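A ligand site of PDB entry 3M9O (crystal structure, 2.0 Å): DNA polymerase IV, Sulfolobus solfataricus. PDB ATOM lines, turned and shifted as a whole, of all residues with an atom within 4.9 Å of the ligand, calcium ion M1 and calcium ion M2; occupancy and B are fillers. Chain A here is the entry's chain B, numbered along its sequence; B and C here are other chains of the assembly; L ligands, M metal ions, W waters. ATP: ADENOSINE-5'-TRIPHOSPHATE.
OG1 of Thr 45 is in hydrogen-bond range of O1B of the ligand. O4 of DT 3 of chain C is in hydrogen-bond range of N6 of the ligand, 2.7 Å away. The side-chain amino group (NZ) of Lys 159 is in salt-bridge range of an oxygen (O1G) of the ligand (3.4 Å). N of Tyr 10 sits at hydrogen-bond distance from O2G of the ligand, 3.0 Å away. An oxygen (O3') of the ligand sits at hydrogen-bond distance from the backbone NH (N) of Tyr 12 of chain A, at 2.9 Å. An oxygen (O2B) of the ligand sits close to the backbone NH of Phe 11 (3.2 Å). An oxygen (O1B) of the ligand lies within salt-bridge range of the guanidinium group of Arg 51 (3.0 Å). The side-chain hydroxyl (OH) of Tyr 48 sits at hydrogen-bond distance from an oxygen (O2G) of the ligand, 2.6 Å away. A nitrogen (N6) of the ligand lies within hydrogen-bond range of N4 of DC 13 of chain B, 3.3 Å away.
The side-chain hydroxyl of Thr 45 lies within hydrogen-bond range of the guanidinium group of Arg 51 (3.5 Å). The side-chain amino group (NZ) of Lys 152 lies close to the side-chain carboxylate (OE2) of Glu 106, 2.7 Å away. OP1 of DC 13 of chain B sits close to the side-chain amino group (NZ) of Lys 152. NZ of Lys 159 lies close to OD2 of Asp 7 (2.9 Å). O of Ala 46 sits at hydrogen-bond distance from NE of Arg 51, 3.1 Å away.
N2 of DG 4 of chain C lies close to a nitrogen (N3) of the ligand, 2.9 Å away. Residues that only touch the ligand: Ala 44, Asp 9 and Ala 57. Hydrophobic or aromatic side chains within 4 Å of the ligand: Phe 11, Tyr 12 of chain A, Ala 44, Tyr 48 and Ala 57. Of the 25 residues printed, 16 come within 4 Å of the ligand. The nearest printed residue that does not touch the ligand is Ile 104 (4.1 Å).
Within 4 Å of calcium ion M1: Asp 7, Phe 8 and Asp 105.
Merely in contact with calcium ion M2: Lys 152 and Lys 159. Within 4 Å of calcium ion M2: Asp 7, Glu 106, Lys 152, Lys 159 and DC 13 of chain B. Along chain A the residues within 4 Å of calcium ion M2 span positions 7 to 159.
Calcium ion M1 is bound by an oxygen (O3G) of the ligand (2.2 Å). OD2 of Asp 105 is bound to calcium ion M1, at 2.4 Å. Calcium ion M1 is bound by an oxygen (O2B) of the ligand (2.4 Å). O of Phe 8 binds calcium ion M1 (2.4 Å). OD1 of Asp 7 binds calcium ion M1, at 2.4 Å. O1A of the ligand binds calcium ion M1 (2.4 Å).
Calcium ion M2 is bound by water W3, 2.4 Å away. OP1 of DC 13 of chain B is bound to calcium ion M2, at 2.4 Å. Water W5 binds calcium ion M2, at 2.5 Å. OE2 of Glu 106 binds calcium ion M2 (2.5 Å). Water W2 binds calcium ion M2 (2.5 Å). The side-chain carboxylate (OD2) of Asp 7 binds calcium ion M2 (2.6 Å). Calcium ion M2 has six donor atoms within binding distance.
Water W5 bridges NZ of Lys 159 (3.0 Å) and O2A of the ligand (3.4 Å). Water W6 lies within hydrogen-bond range of the side-chain hydroxyl (OH) of Tyr 12 of chain A (2.7 Å), N2 of DG 4 of chain C (2.9 Å) and a nitrogen (N3) of the ligand (3.0 Å). Water W7 lies within hydrogen-bond range of the side-chain carboxylate of Asp 9 (2.5 Å) and the backbone carbonyl oxygen of Asp 7 (2.9 Å).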
ATOM      1  N   PHE A   5     -35.169 -11.661  -8.085  1.00  0.00           N
ATOM      2  CA  PHE A   5     -34.440 -12.474  -7.133  1.00  0.00           C
ATOM      3  C   PHE A   5     -35.290 -12.675  -5.897  1.00  0.00           C
ATOM      4  O   PHE A   5     -35.889 -11.710  -5.387  1.00  0.00           O
ATOM      5  CB  PHE A   5     -33.126 -11.753  -6.781  1.00  0.00           C
ATOM      6  CG  PHE A   5     -32.332 -12.404  -5.699  1.00  0.00           C
ATOM      7  CD1 PHE A   5     -31.676 -13.616  -5.910  1.00  0.00           C
ATOM      8  CD2 PHE A   5     -32.166 -11.760  -4.469  1.00  0.00           C
ATOM      9  CE1 PHE A   5     -30.871 -14.176  -4.928  1.00  0.00           C
ATOM     10  CE2 PHE A   5     -31.360 -12.297  -3.449  1.00  0.00           C
ATOM     11  CZ  PHE A   5     -30.701 -13.512  -3.690  1.00  0.00           C
ATOM     12  N   ASP A   7     -35.287 -14.225  -1.950  1.00  0.00           N
ATOM     13  CA  ASP A   7     -34.400 -14.607  -0.867  1.00  0.00           C
ATOM     14  C   ASP A   7     -35.285 -14.813   0.362  1.00  0.00           C
ATOM     15  O   ASP A   7     -35.847 -13.851   0.872  1.00  0.00           O
ATOM     16  CB  ASP A   7     -33.431 -13.464  -0.657  1.00  0.00           C
ATOM     17  CG  ASP A   7     -32.410 -13.755   0.404  1.00  0.00           C
ATOM     18  OD1 ASP A   7     -32.740 -14.425   1.361  1.00  0.00           O
ATOM     19  OD2 ASP A   7     -31.260 -13.301   0.284  1.00  0.00           O
ATOM     20  N   PHE A   8     -35.449 -16.057   0.815  1.00  0.00           N
ATOM     21  CA  PHE A   8     -36.336 -16.357   1.964  1.00  0.00           C
ATOM     22  C   PHE A   8     -35.831 -15.695   3.275  1.00  0.00           C
ATOM     23  O   PHE A   8     -34.629 -15.775   3.610  1.00  0.00           O
ATOM     24  CB  PHE A   8     -36.450 -17.882   2.196  1.00  0.00           C
ATOM     25  CG  PHE A   8     -36.614 -18.712   0.924  1.00  0.00           C
ATOM     26  CD1 PHE A   8     -37.071 -18.148  -0.243  1.00  0.00           C
ATOM     27  CD2 PHE A   8     -36.373 -20.084   0.945  1.00  0.00           C
ATOM     28  CE1 PHE A   8     -37.301 -18.944  -1.413  1.00  0.00           C
ATOM     29  CE2 PHE A   8     -36.584 -20.873  -0.193  1.00  0.00           C
ATOM     30  CZ  PHE A   8     -37.046 -20.305  -1.368  1.00  0.00           C
ATOM     31  N   ASP A   9     -36.743 -15.081   4.052  1.00  0.00           N
ATOM     32  CA  ASP A   9     -36.325 -14.444   5.313  1.00  0.00           C
ATOM     33  C   ASP A   9     -35.972 -15.434   6.448  1.00  0.00           C
ATOM     34  O   ASP A   9     -36.671 -16.397   6.642  1.00  0.00           O
ATOM     35  CB  ASP A   9     -37.446 -13.502   5.818  1.00  0.00           C
ATOM     36  CG  ASP A   9     -37.788 -12.421   4.821  1.00  0.00           C
ATOM     37  OD1 ASP A   9     -36.829 -11.840   4.209  1.00  0.00           O
ATOM     38  OD2 ASP A   9     -39.000 -12.148   4.616  1.00  0.00           O
ATOM     39  N   TYR A  10     -34.929 -15.124   7.231  1.00  0.00           N
ATOM     40  CA  TYR A  10     -34.447 -15.942   8.355  1.00  0.00           C
ATOM     41  C   TYR A  10     -34.864 -17.391   8.205  1.00  0.00           C
ATOM     42  O   TYR A  10     -35.300 -18.039   9.164  1.00  0.00           O
ATOM     43  CB  TYR A  10     -34.949 -15.390   9.703  1.00  0.00           C
ATOM     44  CG  TYR A  10     -36.437 -15.221   9.911  1.00  0.00           C
ATOM     45  CD1 TYR A  10     -37.134 -14.174   9.272  1.00  0.00           C
ATOM     46  CD2 TYR A  10     -37.150 -16.025  10.856  1.00  0.00           C
ATOM     47  CE1 TYR A  10     -38.518 -13.930   9.588  1.00  0.00           C
ATOM     48  CE2 TYR A  10     -38.506 -15.775  11.158  1.00  0.00           C
ATOM     49  CZ  TYR A  10     -39.179 -14.761  10.537  1.00  0.00           C
ATOM     50  OH  TYR A  10     -40.529 -14.565  10.776  1.00  0.00           O
ATOM     51  N   PHE A  11     -34.594 -17.900   7.006  1.00  0.00           N
ATOM     52  CA  PHE A  11     -35.048 -19.203   6.633  1.00  0.00           C
ATOM     53  C   PHE A  11     -35.081 -20.317   7.658  1.00  0.00           C
ATOM     54  O   PHE A  11     -36.153 -20.763   7.982  1.00  0.00           O
ATOM     55  CB  PHE A  11     -34.336 -19.671   5.368  1.00  0.00           C
ATOM     56  CG  PHE A  11     -35.051 -20.822   4.682  1.00  0.00           C
ATOM     57  CD1 PHE A  11     -36.439 -20.816   4.479  1.00  0.00           C
ATOM     58  CD2 PHE A  11     -34.321 -21.944   4.275  1.00  0.00           C
ATOM     59  CE1 PHE A  11     -37.082 -21.894   3.908  1.00  0.00           C
ATOM     60  CE2 PHE A  11     -34.963 -23.021   3.704  1.00  0.00           C
ATOM     61  CZ  PHE A  11     -36.341 -23.008   3.512  1.00  0.00           C
ATOM     62  N   TYR A  12     -33.936 -20.776   8.170  1.00  0.00           N
ATOM     63  CA  TYR A  12     -33.974 -21.886   9.121  1.00  0.00           C
ATOM     64  C   TYR A  12     -34.860 -21.598  10.357  1.00  0.00           C
ATOM     65  O   TYR A  12     -35.669 -22.460  10.801  1.00  0.00           O
ATOM     66  CB  TYR A  12     -32.590 -22.251   9.611  1.00  0.00           C
ATOM     67  CG  TYR A  12     -31.725 -22.943   8.580  1.00  0.00           C
ATOM     68  CD1 TYR A  12     -32.090 -23.002   7.234  1.00  0.00           C
ATOM     69  CD2 TYR A  12     -30.489 -23.469   8.942  1.00  0.00           C
ATOM     70  CE1 TYR A  12     -31.253 -23.568   6.281  1.00  0.00           C
ATOM     71  CE2 TYR A  12     -29.649 -24.021   8.022  1.00  0.00           C
ATOM     72  CZ  TYR A  12     -30.024 -24.076   6.684  1.00  0.00           C
ATOM     73  OH  TYR A  12     -29.158 -24.639   5.754  1.00  0.00           O
ATOM     74  N   VAL A  32     -25.736 -25.532  15.269  1.00  0.00           N
ATOM     75  CA  VAL A  32     -24.998 -26.595  14.599  1.00  0.00           C
ATOM     76  C   VAL A  32     -24.056 -27.066  15.701  1.00  0.00           C
ATOM     77  O   VAL A  32     -22.962 -26.539  15.873  1.00  0.00           O
ATOM     78  CB  VAL A  32     -24.178 -26.099  13.421  1.00  0.00           C
ATOM     79  CG1 VAL A  32     -23.435 -27.286  12.782  1.00  0.00           C
ATOM     80  CG2 VAL A  32     -25.092 -25.427  12.402  1.00  0.00           C
ATOM     81  N   VAL A  43     -23.768 -20.976  15.476  1.00  0.00           N
ATOM     82  CA  VAL A  43     -25.113 -20.616  15.091  1.00  0.00           C
ATOM     83  C   VAL A  43     -25.254 -20.716  13.574  1.00  0.00           C
ATOM     84  O   VAL A  43     -24.433 -20.174  12.845  1.00  0.00           O
ATOM     85  CB  VAL A  43     -25.444 -19.166  15.545  1.00  0.00           C
ATOM     86  CG1 VAL A  43     -26.782 -18.765  15.006  1.00  0.00           C
ATOM     87  CG2 VAL A  43     -25.478 -19.097  17.092  1.00  0.00           C
ATOM     88  N   ALA A  44     -26.267 -21.421  13.089  1.00  0.00           N
ATOM     89  CA  ALA A  44     -26.525 -21.496  11.649  1.00  0.00           C
ATOM     90  C   ALA A  44     -27.256 -20.199  11.229  1.00  0.00           C
ATOM     91  O   ALA A  44     -26.963 -19.598  10.163  1.00  0.00           O
ATOM     92  CB  ALA A  44     -27.397 -22.688  11.335  1.00  0.00           C
ATOM     93  N   THR A  45     -28.222 -19.793  12.041  1.00  0.00           N
ATOM     94  CA  THR A  45     -28.953 -18.568  11.818  1.00  0.00           C
ATOM     95  C   THR A  45     -29.855 -18.283  13.036  1.00  0.00           C
ATOM     96  O   THR A  45     -29.996 -19.108  13.927  1.00  0.00           O
ATOM     97  CB  THR A  45     -29.811 -18.646  10.557  1.00  0.00           C
ATOM     98  OG1 THR A  45     -30.175 -17.320  10.179  1.00  0.00           O
ATOM     99  CG2 THR A  45     -31.051 -19.468  10.776  1.00  0.00           C
ATOM    100  N   ALA A  46     -30.459 -17.105  13.074  1.00  0.00           N
ATOM    101  CA  ALA A  46     -31.356 -16.736  14.165  1.00  0.00           C
ATOM    102  C   ALA A  46     -32.372 -15.783  13.587  1.00  0.00           C
ATOM    103  O   ALA A  46     -32.072 -15.123  12.564  1.00  0.00           O
ATOM    104  CB  ALA A  46     -30.588 -16.031  15.275  1.00  0.00           C
ATOM    105  N   TYR A  48     -34.628 -12.286  13.521  1.00  0.00           N
ATOM    106  CA  TYR A  48     -34.212 -10.914  13.892  1.00  0.00           C
ATOM    107  C   TYR A  48     -34.423 -10.594  15.381  1.00  0.00           C
ATOM    108  O   TYR A  48     -33.697  -9.792  15.938  1.00  0.00           O
ATOM    109  CB  TYR A  48     -34.943  -9.920  13.006  1.00  0.00           C
ATOM    110  CG  TYR A  48     -34.569 -10.014  11.513  1.00  0.00           C
ATOM    111  CD1 TYR A  48     -33.596  -9.190  10.940  1.00  0.00           C
ATOM    112  CD2 TYR A  48     -35.218 -10.907  10.695  1.00  0.00           C
ATOM    113  CE1 TYR A  48     -33.294  -9.268   9.571  1.00  0.00           C
ATOM    114  CE2 TYR A  48     -34.950 -11.021   9.379  1.00  0.00           C
ATOM    115  CZ  TYR A  48     -34.001 -10.205   8.791  1.00  0.00           C
ATOM    116  OH  TYR A  48     -33.741 -10.300   7.413  1.00  0.00           O
ATOM    117  N   ARG A  51     -31.220 -11.723  16.284  1.00  0.00           N
ATOM    118  CA  ARG A  51     -30.178 -11.030  15.537  1.00  0.00           C
ATOM    119  C   ARG A  51     -30.009  -9.572  15.907  1.00  0.00           C
ATOM    120  O   ARG A  51     -28.892  -9.059  15.884  1.00  0.00           O
ATOM    121  CB  ARG A  51     -30.469 -11.094  14.020  1.00  0.00           C
ATOM    122  CG  ARG A  51     -30.296 -12.470  13.460  1.00  0.00           C
ATOM    123  CD  ARG A  51     -29.388 -12.420  12.258  1.00  0.00           C
ATOM    124  NE  ARG A  51     -29.890 -13.395  11.296  1.00  0.00           N
ATOM    125  CZ  ARG A  51     -30.595 -13.078  10.229  1.00  0.00           C
ATOM    126  NH1 ARG A  51     -30.877 -11.812   9.961  1.00  0.00           N
ATOM    127  NH2 ARG A  51     -31.058 -14.045   9.458  1.00  0.00           N
ATOM    128  N   ALA A  57     -25.527 -15.851  12.374  1.00  0.00           N
ATOM    129  CA  ALA A  57     -24.840 -16.971  11.745  1.00  0.00           C
ATOM    130  C   ALA A  57     -23.335 -16.936  11.935  1.00  0.00           C
ATOM    131  O   ALA A  57     -22.676 -15.907  11.725  1.00  0.00           O
ATOM    132  CB  ALA A  57     -25.169 -16.983  10.230  1.00  0.00           C
ATOM    133  N   GLY A  58     -22.791 -18.056  12.394  1.00  0.00           N
ATOM    134  CA  GLY A  58     -21.352 -18.106  12.538  1.00  0.00           C
ATOM    135  C   GLY A  58     -20.766 -17.891  13.910  1.00  0.00           C
ATOM    136  O   GLY A  58     -19.670 -18.341  14.154  1.00  0.00           O
ATOM    137  N   ILE A 104     -29.862 -22.815  -0.918  1.00  0.00           N
ATOM    138  CA  ILE A 104     -31.029 -23.357  -0.229  1.00  0.00           C
ATOM    139  C   ILE A 104     -32.196 -22.380  -0.110  1.00  0.00           C
ATOM    140  O   ILE A 104     -33.344 -22.795   0.043  1.00  0.00           O
ATOM    141  CB  ILE A 104     -30.637 -23.869   1.170  1.00  0.00           C
ATOM    142  CG1 ILE A 104     -31.766 -24.795   1.720  1.00  0.00           C
ATOM    143  CG2 ILE A 104     -30.359 -22.674   2.100  1.00  0.00           C
ATOM    144  CD1 ILE A 104     -31.278 -25.891   2.535  1.00  0.00           C
ATOM    145  N   ASP A 105     -31.933 -21.076  -0.182  1.00  0.00           N
ATOM    146  CA  ASP A 105     -33.016 -20.125  -0.067  1.00  0.00           C
ATOM    147  C   ASP A 105     -32.976 -18.916  -1.028  1.00  0.00           C
ATOM    148  O   ASP A 105     -33.505 -17.844  -0.703  1.00  0.00           O
ATOM    149  CB  ASP A 105     -33.046 -19.655   1.390  1.00  0.00           C
ATOM    150  CG  ASP A 105     -32.027 -18.574   1.651  1.00  0.00           C
ATOM    151  OD1 ASP A 105     -30.954 -18.497   0.967  1.00  0.00           O
ATOM    152  OD2 ASP A 105     -32.306 -17.777   2.584  1.00  0.00           O
ATOM    153  N   GLU A 106     -32.354 -19.085  -2.195  1.00  0.00           N
ATOM    154  CA  GLU A 106     -32.258 -17.995  -3.182  1.00  0.00           C
ATOM    155  C   GLU A 106     -32.524 -18.527  -4.561  1.00  0.00           C
ATOM    156  O   GLU A 106     -32.119 -19.650  -4.915  1.00  0.00           O
ATOM    157  CB  GLU A 106     -30.856 -17.399  -3.212  1.00  0.00           C
ATOM    158  CG  GLU A 106     -30.363 -16.822  -1.929  1.00  0.00           C
ATOM    159  CD  GLU A 106     -28.903 -16.485  -2.054  1.00  0.00           C
ATOM    160  OE1 GLU A 106     -28.125 -17.423  -2.347  1.00  0.00           O
ATOM    161  OE2 GLU A 106     -28.561 -15.298  -1.873  1.00  0.00           O
ATOM    162  N   LYS A 152     -29.898  -8.744  -6.617  1.00  0.00           N
ATOM    163  CA  LYS A 152     -29.504  -9.204  -5.269  1.00  0.00           C
ATOM    164  C   LYS A 152     -29.322  -7.997  -4.323  1.00  0.00           C
ATOM    165  O   LYS A 152     -29.756  -8.029  -3.195  1.00  0.00           O
ATOM    166  CB  LYS A 152     -28.204  -9.983  -5.348  1.00  0.00           C
ATOM    167  CG  LYS A 152     -27.754 -10.641  -4.005  1.00  0.00           C
ATOM    168  CD  LYS A 152     -26.479 -11.451  -4.204  1.00  0.00           C
ATOM    169  CE  LYS A 152     -26.049 -12.175  -2.952  1.00  0.00           C
ATOM    170  NZ  LYS A 152     -27.012 -13.234  -2.574  1.00  0.00           N
ATOM    171  N   LYS A 159     -34.799  -6.467   2.672  1.00  0.00           N
ATOM    172  CA  LYS A 159     -35.121  -7.501   3.640  1.00  0.00           C
ATOM    173  C   LYS A 159     -35.287  -6.989   5.077  1.00  0.00           C
ATOM    174  O   LYS A 159     -34.663  -6.002   5.489  1.00  0.00           O
ATOM    175  CB  LYS A 159     -34.107  -8.676   3.560  1.00  0.00           C
ATOM    176  CG  LYS A 159     -32.671  -8.336   3.746  1.00  0.00           C
ATOM    177  CD  LYS A 159     -31.807  -9.619   3.822  1.00  0.00           C
ATOM    178  CE  LYS A 159     -31.822 -10.400   2.507  1.00  0.00           C
ATOM    179  NZ  LYS A 159     -30.859 -11.567   2.532  1.00  0.00           N
ATOM    180  P    DC B  12     -19.310 -12.167  -0.630  1.00  0.00           P
ATOM    181  OP1  DC B  12     -19.969 -11.010  -1.298  1.00  0.00           O
ATOM    182  OP2  DC B  12     -18.717 -11.975   0.724  1.00  0.00           O
ATOM    183  O5'  DC B  12     -20.335 -13.373  -0.521  1.00  0.00           O
ATOM    184  C5'  DC B  12     -21.004 -13.760  -1.712  1.00  0.00           C
ATOM    185  C4'  DC B  12     -21.839 -14.962  -1.354  1.00  0.00           C
ATOM    186  O4'  DC B  12     -20.962 -16.036  -0.954  1.00  0.00           O
ATOM    187  C3'  DC B  12     -22.729 -14.653  -0.130  1.00  0.00           C
ATOM    188  O3'  DC B  12     -24.108 -14.805  -0.443  1.00  0.00           O
ATOM    189  C2'  DC B  12     -22.279 -15.644   0.941  1.00  0.00           C
ATOM    190  C1'  DC B  12     -21.548 -16.713   0.140  1.00  0.00           C
ATOM    191  N1   DC B  12     -20.512 -17.315   0.973  1.00  0.00           N
ATOM    192  C2   DC B  12     -20.512 -18.707   1.087  1.00  0.00           C
ATOM    193  O2   DC B  12     -21.307 -19.353   0.399  1.00  0.00           O
ATOM    194  N3   DC B  12     -19.652 -19.302   1.933  1.00  0.00           N
ATOM    195  C4   DC B  12     -18.789 -18.573   2.637  1.00  0.00           C
ATOM    196  N4   DC B  12     -17.954 -19.212   3.447  1.00  0.00           N
ATOM    197  C5   DC B  12     -18.744 -17.143   2.541  1.00  0.00           C
ATOM    198  C6   DC B  12     -19.599 -16.564   1.684  1.00  0.00           C
ATOM    199  P    DC B  13     -25.197 -14.713   0.760  1.00  0.00           P
ATOM    200  OP1  DC B  13     -26.367 -14.061   0.202  1.00  0.00           O
ATOM    201  OP2  DC B  13     -24.561 -14.095   1.972  1.00  0.00           O
ATOM    202  O5'  DC B  13     -25.489 -16.231   1.138  1.00  0.00           O
ATOM    203  C5'  DC B  13     -25.942 -17.076   0.073  1.00  0.00           C
ATOM    204  C4'  DC B  13     -26.275 -18.456   0.611  1.00  0.00           C
ATOM    205  O4'  DC B  13     -25.052 -19.137   0.970  1.00  0.00           O
ATOM    206  C3'  DC B  13     -27.204 -18.463   1.850  1.00  0.00           C
ATOM    207  C2'  DC B  13     -26.545 -19.400   2.856  1.00  0.00           C
ATOM    208  C1'  DC B  13     -25.248 -19.902   2.170  1.00  0.00           C
ATOM    209  N1   DC B  13     -24.115 -19.624   3.061  1.00  0.00           N
ATOM    210  C2   DC B  13     -23.682 -20.677   3.816  1.00  0.00           C
ATOM    211  O2   DC B  13     -24.296 -21.763   3.726  1.00  0.00           O
ATOM    212  N3   DC B  13     -22.624 -20.512   4.625  1.00  0.00           N
ATOM    213  C4   DC B  13     -22.011 -19.337   4.715  1.00  0.00           C
ATOM    214  N4   DC B  13     -20.979 -19.226   5.536  1.00  0.00           N
ATOM    215  C5   DC B  13     -22.437 -18.205   3.961  1.00  0.00           C
ATOM    216  C6   DC B  13     -23.495 -18.395   3.150  1.00  0.00           C
ATOM    217  P    DT C   3     -16.212 -24.856  13.661  1.00  0.00           P
ATOM    218  OP1  DT C   3     -15.460 -25.637  14.696  1.00  0.00           O
ATOM    219  OP2  DT C   3     -15.632 -24.673  12.300  1.00  0.00           O
ATOM    220  O5'  DT C   3     -17.678 -25.467  13.552  1.00  0.00           O
ATOM    221  C5'  DT C   3     -18.405 -25.878  14.719  1.00  0.00           C
ATOM    222  C4'  DT C   3     -19.615 -26.625  14.219  1.00  0.00           C
ATOM    223  O4'  DT C   3     -20.508 -25.674  13.586  1.00  0.00           O
ATOM    224  C3'  DT C   3     -19.245 -27.615  13.115  1.00  0.00           C
ATOM    225  O3'  DT C   3     -20.188 -28.685  13.090  1.00  0.00           O
ATOM    226  C2'  DT C   3     -19.372 -26.775  11.852  1.00  0.00           C
ATOM    227  C1'  DT C   3     -20.592 -25.913  12.190  1.00  0.00           C
ATOM    228  N1   DT C   3     -20.570 -24.598  11.540  1.00  0.00           N
ATOM    229  C2   DT C   3     -21.591 -24.248  10.672  1.00  0.00           C
ATOM    230  O2   DT C   3     -22.515 -24.978  10.339  1.00  0.00           O
ATOM    231  N3   DT C   3     -21.477 -22.979  10.187  1.00  0.00           N
ATOM    232  C4   DT C   3     -20.499 -22.052  10.466  1.00  0.00           C
ATOM    233  O4   DT C   3     -20.563 -20.937   9.982  1.00  0.00           O
ATOM    234  C5   DT C   3     -19.478 -22.498  11.358  1.00  0.00           C
ATOM    235  C7   DT C   3     -18.374 -21.552  11.725  1.00  0.00           C
ATOM    236  C6   DT C   3     -19.553 -23.736  11.835  1.00  0.00           C
ATOM    237  P    DG C   4     -19.768 -30.094  12.442  1.00  0.00           P
ATOM    238  OP1  DG C   4     -20.438 -31.214  13.058  1.00  0.00           O
ATOM    239  OP2  DG C   4     -18.361 -30.269  12.230  1.00  0.00           O
ATOM    240  O5'  DG C   4     -20.591 -30.072  11.163  1.00  0.00           O
ATOM    241  C5'  DG C   4     -20.292 -29.178  10.288  1.00  0.00           C
ATOM    242  C4'  DG C   4     -21.417 -29.029   9.293  1.00  0.00           C
ATOM    243  O4'  DG C   4     -21.574 -27.605   9.114  1.00  0.00           O
ATOM    244  C3'  DG C   4     -21.007 -29.744   8.043  1.00  0.00           C
ATOM    245  O3'  DG C   4     -22.053 -30.300   7.280  1.00  0.00           O
ATOM    246  C2'  DG C   4     -20.220 -28.577   7.458  1.00  0.00           C
ATOM    247  C1'  DG C   4     -21.146 -27.342   7.951  1.00  0.00           C
ATOM    248  N9   DG C   4     -20.445 -26.017   7.738  1.00  0.00           N
ATOM    249  C8   DG C   4     -19.081 -25.673   7.893  1.00  0.00           C
ATOM    250  N7   DG C   4     -18.755 -24.430   7.533  1.00  0.00           N
ATOM    251  C5   DG C   4     -20.065 -23.940   7.107  1.00  0.00           C
ATOM    252  C6   DG C   4     -20.508 -22.676   6.612  1.00  0.00           C
ATOM    253  O6   DG C   4     -19.840 -21.685   6.440  1.00  0.00           O
ATOM    254  N1   DG C   4     -21.902 -22.648   6.293  1.00  0.00           N
ATOM    255  C2   DG C   4     -22.771 -23.700   6.441  1.00  0.00           C
ATOM    256  N2   DG C   4     -24.043 -23.499   6.089  1.00  0.00           N
ATOM    257  N3   DG C   4     -22.389 -24.863   6.915  1.00  0.00           N
ATOM    258  C4   DG C   4     -21.052 -24.925   7.225  1.00  0.00           C
HETATM  259  PG  ATP L   1     -31.799 -13.211   5.940  1.00  0.00           P
HETATM  260  O1G ATP L   1     -30.599 -12.133   5.895  1.00  0.00           O
HETATM  261  O2G ATP L   1     -33.116 -12.776   6.707  1.00  0.00           O
HETATM  262  O3G ATP L   1     -32.127 -13.653   4.521  1.00  0.00           O
HETATM  263  PB  ATP L   1     -31.204 -16.019   6.787  1.00  0.00           P
HETATM  264  O1B ATP L   1     -31.413 -16.664   8.130  1.00  0.00           O
HETATM  265  O2B ATP L   1     -32.115 -16.468   5.626  1.00  0.00           O
HETATM  266  O3B ATP L   1     -31.113 -14.427   6.901  1.00  0.00           O
HETATM  267  PA  ATP L   1     -28.957 -16.168   4.940  1.00  0.00           P
HETATM  268  O1A ATP L   1     -29.889 -15.622   3.980  1.00  0.00           O
HETATM  269  O2A ATP L   1     -27.607 -15.526   5.170  1.00  0.00           O
HETATM  270  O3A ATP L   1     -29.676 -16.348   6.381  1.00  0.00           O
HETATM  271  O5' ATP L   1     -28.719 -17.679   4.565  1.00  0.00           O
HETATM  272  C5' ATP L   1     -29.812 -18.534   4.337  1.00  0.00           C
HETATM  273  C4' ATP L   1     -29.861 -19.754   5.258  1.00  0.00           C
HETATM  274  O4' ATP L   1     -28.702 -20.563   5.135  1.00  0.00           O
HETATM  275  C3' ATP L   1     -30.093 -19.493   6.767  1.00  0.00           C
HETATM  276  O3' ATP L   1     -31.357 -19.766   7.250  1.00  0.00           O
HETATM  277  C2' ATP L   1     -29.029 -20.268   7.482  1.00  0.00           C
HETATM  278  C1' ATP L   1     -28.145 -20.929   6.417  1.00  0.00           C
HETATM  279  N9  ATP L   1     -26.787 -20.372   6.712  1.00  0.00           N
HETATM  280  C8  ATP L   1     -26.324 -19.154   6.367  1.00  0.00           C
HETATM  281  N7  ATP L   1     -25.099 -18.962   6.844  1.00  0.00           N
HETATM  282  C5  ATP L   1     -24.726 -20.070   7.514  1.00  0.00           C
HETATM  283  C6  ATP L   1     -23.546 -20.518   8.314  1.00  0.00           C
HETATM  284  N6  ATP L   1     -22.458 -19.700   8.472  1.00  0.00           N
HETATM  285  N1  ATP L   1     -23.580 -21.779   8.871  1.00  0.00           N
HETATM  286  C2  ATP L   1     -24.644 -22.595   8.753  1.00  0.00           C
HETATM  287  N3  ATP L   1     -25.742 -22.243   8.042  1.00  0.00           N
HETATM  288  C4  ATP L   1     -25.848 -20.995   7.436  1.00  0.00           C
HETATM  289 CA    CA M   1     -32.267 -15.563   3.434  1.00  0.00          CA
HETATM  290 CA    CA M   2     -28.807 -14.079   0.315  1.00  0.00          CA
HETATM  291  O   HOH W   1     -21.548 -16.802   8.032  1.00  0.00           O
HETATM  292  O   HOH W   2     -29.611 -16.279   1.312  1.00  0.00           O
HETATM  293  O   HOH W   3     -28.482 -11.722  -0.146  1.00  0.00           O
HETATM  294  O   HOH W   4     -27.920 -12.956   6.203  1.00  0.00           O
HETATM  295  O   HOH W   5     -28.418 -13.341   2.674  1.00  0.00           O
HETATM  296  O   HOH W   6     -26.635 -24.683   6.639  1.00  0.00           O
HETATM  297  O   HOH W   7     -34.650 -12.328   3.008  1.00  0.00           O
HETATM  298  O   HOH W   8     -23.750 -16.534   6.881  1.00  0.00           O
